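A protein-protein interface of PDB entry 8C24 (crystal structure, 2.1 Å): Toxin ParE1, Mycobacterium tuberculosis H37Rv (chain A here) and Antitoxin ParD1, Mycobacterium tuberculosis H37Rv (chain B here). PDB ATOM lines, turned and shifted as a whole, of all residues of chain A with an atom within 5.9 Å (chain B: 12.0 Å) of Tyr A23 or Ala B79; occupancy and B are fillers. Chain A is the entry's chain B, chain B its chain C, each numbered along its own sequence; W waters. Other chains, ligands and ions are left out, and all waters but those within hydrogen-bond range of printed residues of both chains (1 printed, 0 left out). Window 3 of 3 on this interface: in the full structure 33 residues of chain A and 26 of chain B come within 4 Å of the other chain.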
ATOM      1  N   ILE A  18      -9.351  19.220  -5.073  1.00  0.00           N
ATOM      2  CA  ILE A  18      -9.235  20.530  -4.428  1.00  0.00           C
ATOM      3  C   ILE A  18     -10.616  21.111  -4.143  1.00  0.00           C
ATOM      4  O   ILE A  18     -10.929  21.471  -3.002  1.00  0.00           O
ATOM      5  CB  ILE A  18      -8.395  21.485  -5.292  1.00  0.00           C
ATOM      6  CG1 ILE A  18      -6.986  20.920  -5.471  1.00  0.00           C
ATOM      7  CG2 ILE A  18      -8.347  22.868  -4.650  1.00  0.00           C
ATOM      8  CD1 ILE A  18      -6.160  21.673  -6.476  1.00  0.00           C
ATOM      9  N   TRP A  19     -11.460  21.210  -5.177  1.00  0.00           N
ATOM     10  CA  TRP A  19     -12.828  21.687  -4.977  1.00  0.00           C
ATOM     11  C   TRP A  19     -13.507  20.955  -3.822  1.00  0.00           C
ATOM     12  O   TRP A  19     -13.989  21.583  -2.872  1.00  0.00           O
ATOM     13  CB  TRP A  19     -13.641  21.522  -6.262  1.00  0.00           C
ATOM     14  CG  TRP A  19     -14.879  22.381  -6.310  1.00  0.00           C
ATOM     15  CD1 TRP A  19     -15.039  23.546  -7.009  1.00  0.00           C
ATOM     16  CD2 TRP A  19     -16.133  22.138  -5.651  1.00  0.00           C
ATOM     17  NE1 TRP A  19     -16.307  24.049  -6.817  1.00  0.00           N
ATOM     18  CE2 TRP A  19     -16.998  23.205  -5.988  1.00  0.00           C
ATOM     19  CE3 TRP A  19     -16.606  21.130  -4.799  1.00  0.00           C
ATOM     20  CZ2 TRP A  19     -18.312  23.291  -5.507  1.00  0.00           C
ATOM     21  CZ3 TRP A  19     -17.914  21.217  -4.323  1.00  0.00           C
ATOM     22  CH2 TRP A  19     -18.747  22.293  -4.674  1.00  0.00           C
ATOM     23  N   ASP A  20     -13.544  19.619  -3.887  1.00  0.00           N
ATOM     24  CA  ASP A  20     -14.240  18.840  -2.861  1.00  0.00           C
ATOM     25  C   ASP A  20     -13.648  19.076  -1.481  1.00  0.00           C
ATOM     26  O   ASP A  20     -14.386  19.218  -0.498  1.00  0.00           O
ATOM     27  CB  ASP A  20     -14.186  17.353  -3.196  1.00  0.00           C
ATOM     28  CG  ASP A  20     -14.902  17.024  -4.470  1.00  0.00           C
ATOM     29  OD1 ASP A  20     -15.760  17.827  -4.908  1.00  0.00           O
ATOM     30  OD2 ASP A  20     -14.613  15.955  -5.039  1.00  0.00           O
ATOM     31  N   CYS A  21     -12.321  19.097  -1.382  1.00  0.00           N
ATOM     32  CA  CYS A  21     -11.687  19.348  -0.092  1.00  0.00           C
ATOM     33  C   CYS A  21     -12.057  20.729   0.446  1.00  0.00           C
ATOM     34  O   CYS A  21     -12.346  20.886   1.640  1.00  0.00           O
ATOM     35  CB  CYS A  21     -10.170  19.216  -0.224  1.00  0.00           C
ATOM     36  SG  CYS A  21      -9.296  19.835   1.222  1.00  0.00           S
ATOM     37  N   THR A  22     -12.052  21.739  -0.426  1.00  0.00           N
ATOM     38  CA  THR A  22     -12.389  23.095  -0.009  1.00  0.00           C
ATOM     39  C   THR A  22     -13.862  23.202   0.364  1.00  0.00           C
ATOM     40  O   THR A  22     -14.212  23.881   1.338  1.00  0.00           O
ATOM     41  CB  THR A  22     -12.042  24.079  -1.125  1.00  0.00           C
ATOM     42  OG1 THR A  22     -10.686  23.858  -1.541  1.00  0.00           O
ATOM     43  CG2 THR A  22     -12.171  25.509  -0.633  1.00  0.00           C
ATOM     44  N   TYR A  23     -14.737  22.536  -0.399  1.00  0.00           N
ATOM     45  CA  TYR A  23     -16.164  22.536  -0.082  1.00  0.00           C
ATOM     46  C   TYR A  23     -16.412  21.977   1.315  1.00  0.00           C
ATOM     47  O   TYR A  23     -17.145  22.577   2.115  1.00  0.00           O
ATOM     48  CB  TYR A  23     -16.939  21.728  -1.128  1.00  0.00           C
ATOM     49  CG  TYR A  23     -18.424  21.618  -0.831  1.00  0.00           C
ATOM     50  CD1 TYR A  23     -19.312  22.582  -1.277  1.00  0.00           C
ATOM     51  CD2 TYR A  23     -18.933  20.555  -0.096  1.00  0.00           C
ATOM     52  CE1 TYR A  23     -20.663  22.495  -1.000  1.00  0.00           C
ATOM     53  CE2 TYR A  23     -20.286  20.463   0.190  1.00  0.00           C
ATOM     54  CZ  TYR A  23     -21.144  21.434  -0.265  1.00  0.00           C
ATOM     55  OH  TYR A  23     -22.490  21.340   0.010  1.00  0.00           O
ATOM     56  N   ASP A  24     -15.795  20.830   1.627  1.00  0.00           N
ATOM     57  CA  ASP A  24     -16.033  20.174   2.909  1.00  0.00           C
ATOM     58  C   ASP A  24     -15.589  21.054   4.062  1.00  0.00           C
ATOM     59  O   ASP A  24     -16.272  21.142   5.091  1.00  0.00           O
ATOM     60  CB  ASP A  24     -15.303  18.830   2.964  1.00  0.00           C
ATOM     61  CG  ASP A  24     -15.853  17.818   1.972  1.00  0.00           C
ATOM     62  OD1 ASP A  24     -16.862  18.118   1.297  1.00  0.00           O
ATOM     63  OD2 ASP A  24     -15.263  16.720   1.859  1.00  0.00           O
ATOM     64  N   ARG A  25     -14.448  21.720   3.906  1.00  0.00           N
ATOM     65  CA  ARG A  25     -13.931  22.559   4.976  1.00  0.00           C
ATOM     66  C   ARG A  25     -14.617  23.927   5.011  1.00  0.00           C
ATOM     67  O   ARG A  25     -14.913  24.440   6.094  1.00  0.00           O
ATOM     68  CB  ARG A  25     -12.415  22.695   4.827  1.00  0.00           C
ATOM     69  CG  ARG A  25     -11.785  23.761   5.697  1.00  0.00           C
ATOM     70  CD  ARG A  25     -11.662  23.374   7.156  1.00  0.00           C
ATOM     71  NE  ARG A  25     -12.131  24.434   8.060  1.00  0.00           N
ATOM     72  CZ  ARG A  25     -11.538  24.776   9.206  1.00  0.00           C
ATOM     73  NH1 ARG A  25     -10.440  24.150   9.614  1.00  0.00           N
ATOM     74  NH2 ARG A  25     -12.041  25.756   9.946  1.00  0.00           N
ATOM     75  N   TRP A  26     -14.921  24.519   3.849  1.00  0.00           N
ATOM     76  CA  TRP A  26     -15.295  25.928   3.808  1.00  0.00           C
ATOM     77  C   TRP A  26     -16.585  26.258   3.065  1.00  0.00           C
ATOM     78  O   TRP A  26     -16.997  27.419   3.106  1.00  0.00           O
ATOM     79  CB  TRP A  26     -14.170  26.771   3.180  1.00  0.00           C
ATOM     80  CG  TRP A  26     -12.825  26.669   3.833  1.00  0.00           C
ATOM     81  CD1 TRP A  26     -11.702  26.096   3.307  1.00  0.00           C
ATOM     82  CD2 TRP A  26     -12.448  27.178   5.118  1.00  0.00           C
ATOM     83  NE1 TRP A  26     -10.654  26.208   4.188  1.00  0.00           N
ATOM     84  CE2 TRP A  26     -11.083  26.869   5.306  1.00  0.00           C
ATOM     85  CE3 TRP A  26     -13.129  27.864   6.127  1.00  0.00           C
ATOM     86  CZ2 TRP A  26     -10.395  27.213   6.463  1.00  0.00           C
ATOM     87  CZ3 TRP A  26     -12.442  28.204   7.272  1.00  0.00           C
ATOM     88  CH2 TRP A  26     -11.090  27.880   7.431  1.00  0.00           C
ATOM     89  N   GLY A  27     -17.219  25.317   2.367  1.00  0.00           N
ATOM     90  CA  GLY A  27     -18.459  25.623   1.669  1.00  0.00           C
ATOM     91  C   GLY A  27     -18.252  25.926   0.193  1.00  0.00           C
ATOM     92  O   GLY A  27     -17.128  26.017  -0.317  1.00  0.00           O
ATOM     93  N   VAL A  28     -19.387  26.105  -0.494  1.00  0.00           N
ATOM     94  CA  VAL A  28     -19.411  26.079  -1.954  1.00  0.00           C
ATOM     95  C   VAL A  28     -18.789  27.331  -2.564  1.00  0.00           C
ATOM     96  O   VAL A  28     -18.135  27.247  -3.610  1.00  0.00           O
ATOM     97  CB  VAL A  28     -20.853  25.861  -2.468  1.00  0.00           C
ATOM     98  CG1 VAL A  28     -21.716  27.105  -2.280  1.00  0.00           C
ATOM     99  CG2 VAL A  28     -20.844  25.436  -3.933  1.00  0.00           C
ATOM    100  N   ALA A  31     -15.062  27.128  -2.244  1.00  0.00           N
ATOM    101  CA  ALA A  31     -14.628  26.132  -3.219  1.00  0.00           C
ATOM    102  C   ALA A  31     -14.535  26.733  -4.615  1.00  0.00           C
ATOM    103  O   ALA A  31     -13.534  26.554  -5.321  1.00  0.00           O
ATOM    104  CB  ALA A  31     -15.584  24.937  -3.207  1.00  0.00           C
ATOM    105  N   GLY B  70     -18.371  24.841 -16.961  1.00  0.00           N
ATOM    106  CA  GLY B  70     -19.131  23.612 -16.825  1.00  0.00           C
ATOM    107  C   GLY B  70     -18.743  22.824 -15.595  1.00  0.00           C
ATOM    108  O   GLY B  70     -19.607  22.343 -14.856  1.00  0.00           O
ATOM    109  N   PHE B  71     -17.435  22.697 -15.344  1.00  0.00           N
ATOM    110  CA  PHE B  71     -16.978  21.968 -14.163  1.00  0.00           C
ATOM    111  C   PHE B  71     -17.479  22.627 -12.886  1.00  0.00           C
ATOM    112  O   PHE B  71     -18.012  21.953 -11.994  1.00  0.00           O
ATOM    113  CB  PHE B  71     -15.455  21.868 -14.167  1.00  0.00           C
ATOM    114  CG  PHE B  71     -14.859  21.548 -12.817  1.00  0.00           C
ATOM    115  CD1 PHE B  71     -14.913  20.259 -12.307  1.00  0.00           C
ATOM    116  CD2 PHE B  71     -14.240  22.538 -12.065  1.00  0.00           C
ATOM    117  CE1 PHE B  71     -14.363  19.957 -11.066  1.00  0.00           C
ATOM    118  CE2 PHE B  71     -13.679  22.246 -10.822  1.00  0.00           C
ATOM    119  CZ  PHE B  71     -13.739  20.948 -10.323  1.00  0.00           C
ATOM    120  N   LEU B  72     -17.314  23.949 -12.775  1.00  0.00           N
ATOM    121  CA  LEU B  72     -17.785  24.647 -11.581  1.00  0.00           C
ATOM    122  C   LEU B  72     -19.306  24.606 -11.478  1.00  0.00           C
ATOM    123  O   LEU B  72     -19.851  24.412 -10.383  1.00  0.00           O
ATOM    124  CB  LEU B  72     -17.277  26.088 -11.579  1.00  0.00           C
ATOM    125  CG  LEU B  72     -15.772  26.083 -11.314  1.00  0.00           C
ATOM    126  CD1 LEU B  72     -15.163  27.456 -11.532  1.00  0.00           C
ATOM    127  CD2 LEU B  72     -15.487  25.548  -9.918  1.00  0.00           C
ATOM    128  N   GLY B  73     -20.001  24.775 -12.606  1.00  0.00           N
ATOM    129  CA  GLY B  73     -21.453  24.631 -12.607  1.00  0.00           C
ATOM    130  C   GLY B  73     -21.908  23.276 -12.094  1.00  0.00           C
ATOM    131  O   GLY B  73     -22.739  23.193 -11.184  1.00  0.00           O
ATOM    132  N   ARG B  74     -21.352  22.194 -12.662  1.00  0.00           N
ATOM    133  CA  ARG B  74     -21.721  20.845 -12.240  1.00  0.00           C
ATOM    134  C   ARG B  74     -21.466  20.627 -10.758  1.00  0.00           C
ATOM    135  O   ARG B  74     -22.295  20.037 -10.055  1.00  0.00           O
ATOM    136  CB  ARG B  74     -20.945  19.793 -13.039  1.00  0.00           C
ATOM    137  CG  ARG B  74     -20.761  18.484 -12.249  1.00  0.00           C
ATOM    138  CD  ARG B  74     -20.246  17.321 -13.083  1.00  0.00           C
ATOM    139  NE  ARG B  74     -18.888  17.528 -13.582  1.00  0.00           N
ATOM    140  CZ  ARG B  74     -17.790  17.172 -12.920  1.00  0.00           C
ATOM    141  NH1 ARG B  74     -17.895  16.604 -11.725  1.00  0.00           N
ATOM    142  NH2 ARG B  74     -16.588  17.388 -13.448  1.00  0.00           N
ATOM    143  N   LYS B  75     -20.302  21.063 -10.269  1.00  0.00           N
ATOM    144  CA  LYS B  75     -19.961  20.812  -8.877  1.00  0.00           C
ATOM    145  C   LYS B  75     -20.896  21.574  -7.940  1.00  0.00           C
ATOM    146  O   LYS B  75     -21.377  21.019  -6.947  1.00  0.00           O
ATOM    147  CB  LYS B  75     -18.499  21.176  -8.641  1.00  0.00           C
ATOM    148  CG  LYS B  75     -17.540  20.025  -8.915  1.00  0.00           C
ATOM    149  CD  LYS B  75     -17.440  19.160  -7.675  1.00  0.00           C
ATOM    150  CE  LYS B  75     -16.999  17.768  -7.985  1.00  0.00           C
ATOM    151  NZ  LYS B  75     -16.914  16.983  -6.731  1.00  0.00           N
ATOM    152  N   ARG B  76     -21.189  22.836  -8.252  1.00  0.00           N
ATOM    153  CA  ARG B  76     -22.162  23.569  -7.444  1.00  0.00           C
ATOM    154  C   ARG B  76     -23.516  22.867  -7.460  1.00  0.00           C
ATOM    155  O   ARG B  76     -24.115  22.626  -6.403  1.00  0.00           O
ATOM    156  CB  ARG B  76     -22.304  25.011  -7.940  1.00  0.00           C
ATOM    157  CG  ARG B  76     -23.384  25.804  -7.200  1.00  0.00           C
ATOM    158  CD  ARG B  76     -23.418  27.250  -7.646  1.00  0.00           C
ATOM    159  NE  ARG B  76     -22.309  28.035  -7.107  1.00  0.00           N
ATOM    160  CZ  ARG B  76     -22.264  28.531  -5.870  1.00  0.00           C
ATOM    161  NH1 ARG B  76     -23.261  28.311  -5.022  1.00  0.00           N
ATOM    162  NH2 ARG B  76     -21.218  29.244  -5.474  1.00  0.00           N
ATOM    163  N   ALA B  77     -23.994  22.501  -8.655  1.00  0.00           N
ATOM    164  CA  ALA B  77     -25.278  21.808  -8.779  1.00  0.00           C
ATOM    165  C   ALA B  77     -25.321  20.558  -7.908  1.00  0.00           C
ATOM    166  O   ALA B  77     -26.269  20.356  -7.138  1.00  0.00           O
ATOM    167  CB  ALA B  77     -25.544  21.458 -10.247  1.00  0.00           C
ATOM    168  N   ASP B  78     -24.278  19.724  -7.994  1.00  0.00           N
ATOM    169  CA  ASP B  78     -24.224  18.489  -7.211  1.00  0.00           C
ATOM    170  C   ASP B  78     -24.380  18.760  -5.720  1.00  0.00           C
ATOM    171  O   ASP B  78     -25.142  18.075  -5.029  1.00  0.00           O
ATOM    172  CB  ASP B  78     -22.911  17.752  -7.482  1.00  0.00           C
ATOM    173  CG  ASP B  78     -22.933  16.993  -8.786  1.00  0.00           C
ATOM    174  OD1 ASP B  78     -24.036  16.823  -9.354  1.00  0.00           O
ATOM    175  OD2 ASP B  78     -21.850  16.577  -9.248  1.00  0.00           O
ATOM    176  N   ALA B  79     -23.650  19.746  -5.197  1.00  0.00           N
ATOM    177  CA  ALA B  79     -23.777  20.057  -3.779  1.00  0.00           C
ATOM    178  C   ALA B  79     -25.192  20.504  -3.432  1.00  0.00           C
ATOM    179  O   ALA B  79     -25.676  20.235  -2.326  1.00  0.00           O
ATOM    180  CB  ALA B  79     -22.756  21.123  -3.386  1.00  0.00           C
ATOM    181  N   SER B  80     -25.878  21.162  -4.370  1.00  0.00           N
ATOM    182  CA  SER B  80     -27.266  21.572  -4.177  1.00  0.00           C
ATOM    183  C   SER B  80     -28.247  20.403  -4.126  1.00  0.00           C
ATOM    184  O   SER B  80     -29.404  20.611  -3.743  1.00  0.00           O
ATOM    185  CB  SER B  80     -27.672  22.532  -5.296  1.00  0.00           C
ATOM    186  OG  SER B  80     -29.047  22.377  -5.607  1.00  0.00           O
ATOM    187  N   ARG B  81     -27.834  19.193  -4.510  1.00  0.00           N
ATOM    188  CA  ARG B  81     -28.770  18.070  -4.557  1.00  0.00           C
ATOM    189  C   ARG B  81     -29.061  17.528  -3.162  1.00  0.00           C
ATOM    190  O   ARG B  81     -30.203  17.578  -2.689  1.00  0.00           O
ATOM    191  CB  ARG B  81     -28.220  16.958  -5.455  1.00  0.00           C
ATOM    192  CG  ARG B  81     -28.164  17.321  -6.922  1.00  0.00           C
ATOM    193  CD  ARG B  81     -27.631  16.155  -7.720  1.00  0.00           C
ATOM    194  NE  ARG B  81     -28.568  15.035  -7.772  1.00  0.00           N
ATOM    195  CZ  ARG B  81     -29.382  14.789  -8.801  1.00  0.00           C
ATOM    196  NH1 ARG B  81     -29.378  15.595  -9.861  1.00  0.00           N
ATOM    197  NH2 ARG B  81     -30.196  13.736  -8.779  1.00  0.00           N
HETATM  198  O   HOH W   1     -18.458  25.555  -8.064  1.00  0.00           O
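The side-chain carboxylate (OD2) of Asp A20 is in salt-bridge range of the side-chain amino group (NZ) of Lys B75, 3.0 Å away.
Trp A19 touches Leu B72. Trp A19 touches Lys B75 (CE3 to CD, 3.6 Å). Tyr A23 touches Ala B79 (OH to CB, 3.4 Å). Arg B76 touches Val A28.
Of the printed residues of chain B, Trp A19 touches Leu B72 (3.5 Å) and Lys B75 (3.6 Å). No residue of chain B comes within 4 Å of Cys A21. No residue of chain B comes within 4 Å of Thr A22. Printed residues of chain B within 4 Å of Tyr A23: Ala B79 (3.4 Å). No residue of chain B comes within 4 Å of Asp A24. Arg A25 touches none of the printed residues of chain B. No residue of chain B comes within 4 Å of Gly A27. Of chain B, only Arg B76 comes within 4 Å of Val A28. Of the printed residues of chain A, Leu B72 touches Trp A19 (3.5 Å). Arg B74 touches none of the printed residues of chain A. Of the printed residues of chain A, Lys B75 touches Trp A19 (3.6 Å) and Asp A20 (2.3 Å). Of the printed residues of chain A, Arg B76 touches Val A28. Of chain A, only Tyr A23 comes within 4 Å of Ala B79.
Printed residues of chain A that touch a printed residue of chain B: Trp A19, Asp A20, Tyr A23 and Val A28. Hydrophobic or aromatic side chains of chain A within 4 Å of the printed part of chain B: Trp A19, Tyr A23 and Val A28. Of the 12 printed residues of chain B, 4 touch a printed residue of chain A. Printed residues of chain B that touch a printed residue of chain A: Leu B72, Lys B75, Arg B76 and Ala B79. Among the printed residues, Asp or Glu carboxylates within 4 Å of a Lys or Arg side-chain nitrogen of the other chain: Asp A20 with Lys B75.
Water W1 bridges NE1 of Trp A19 (2.9 Å) and O of Leu B72 (2.9 Å).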
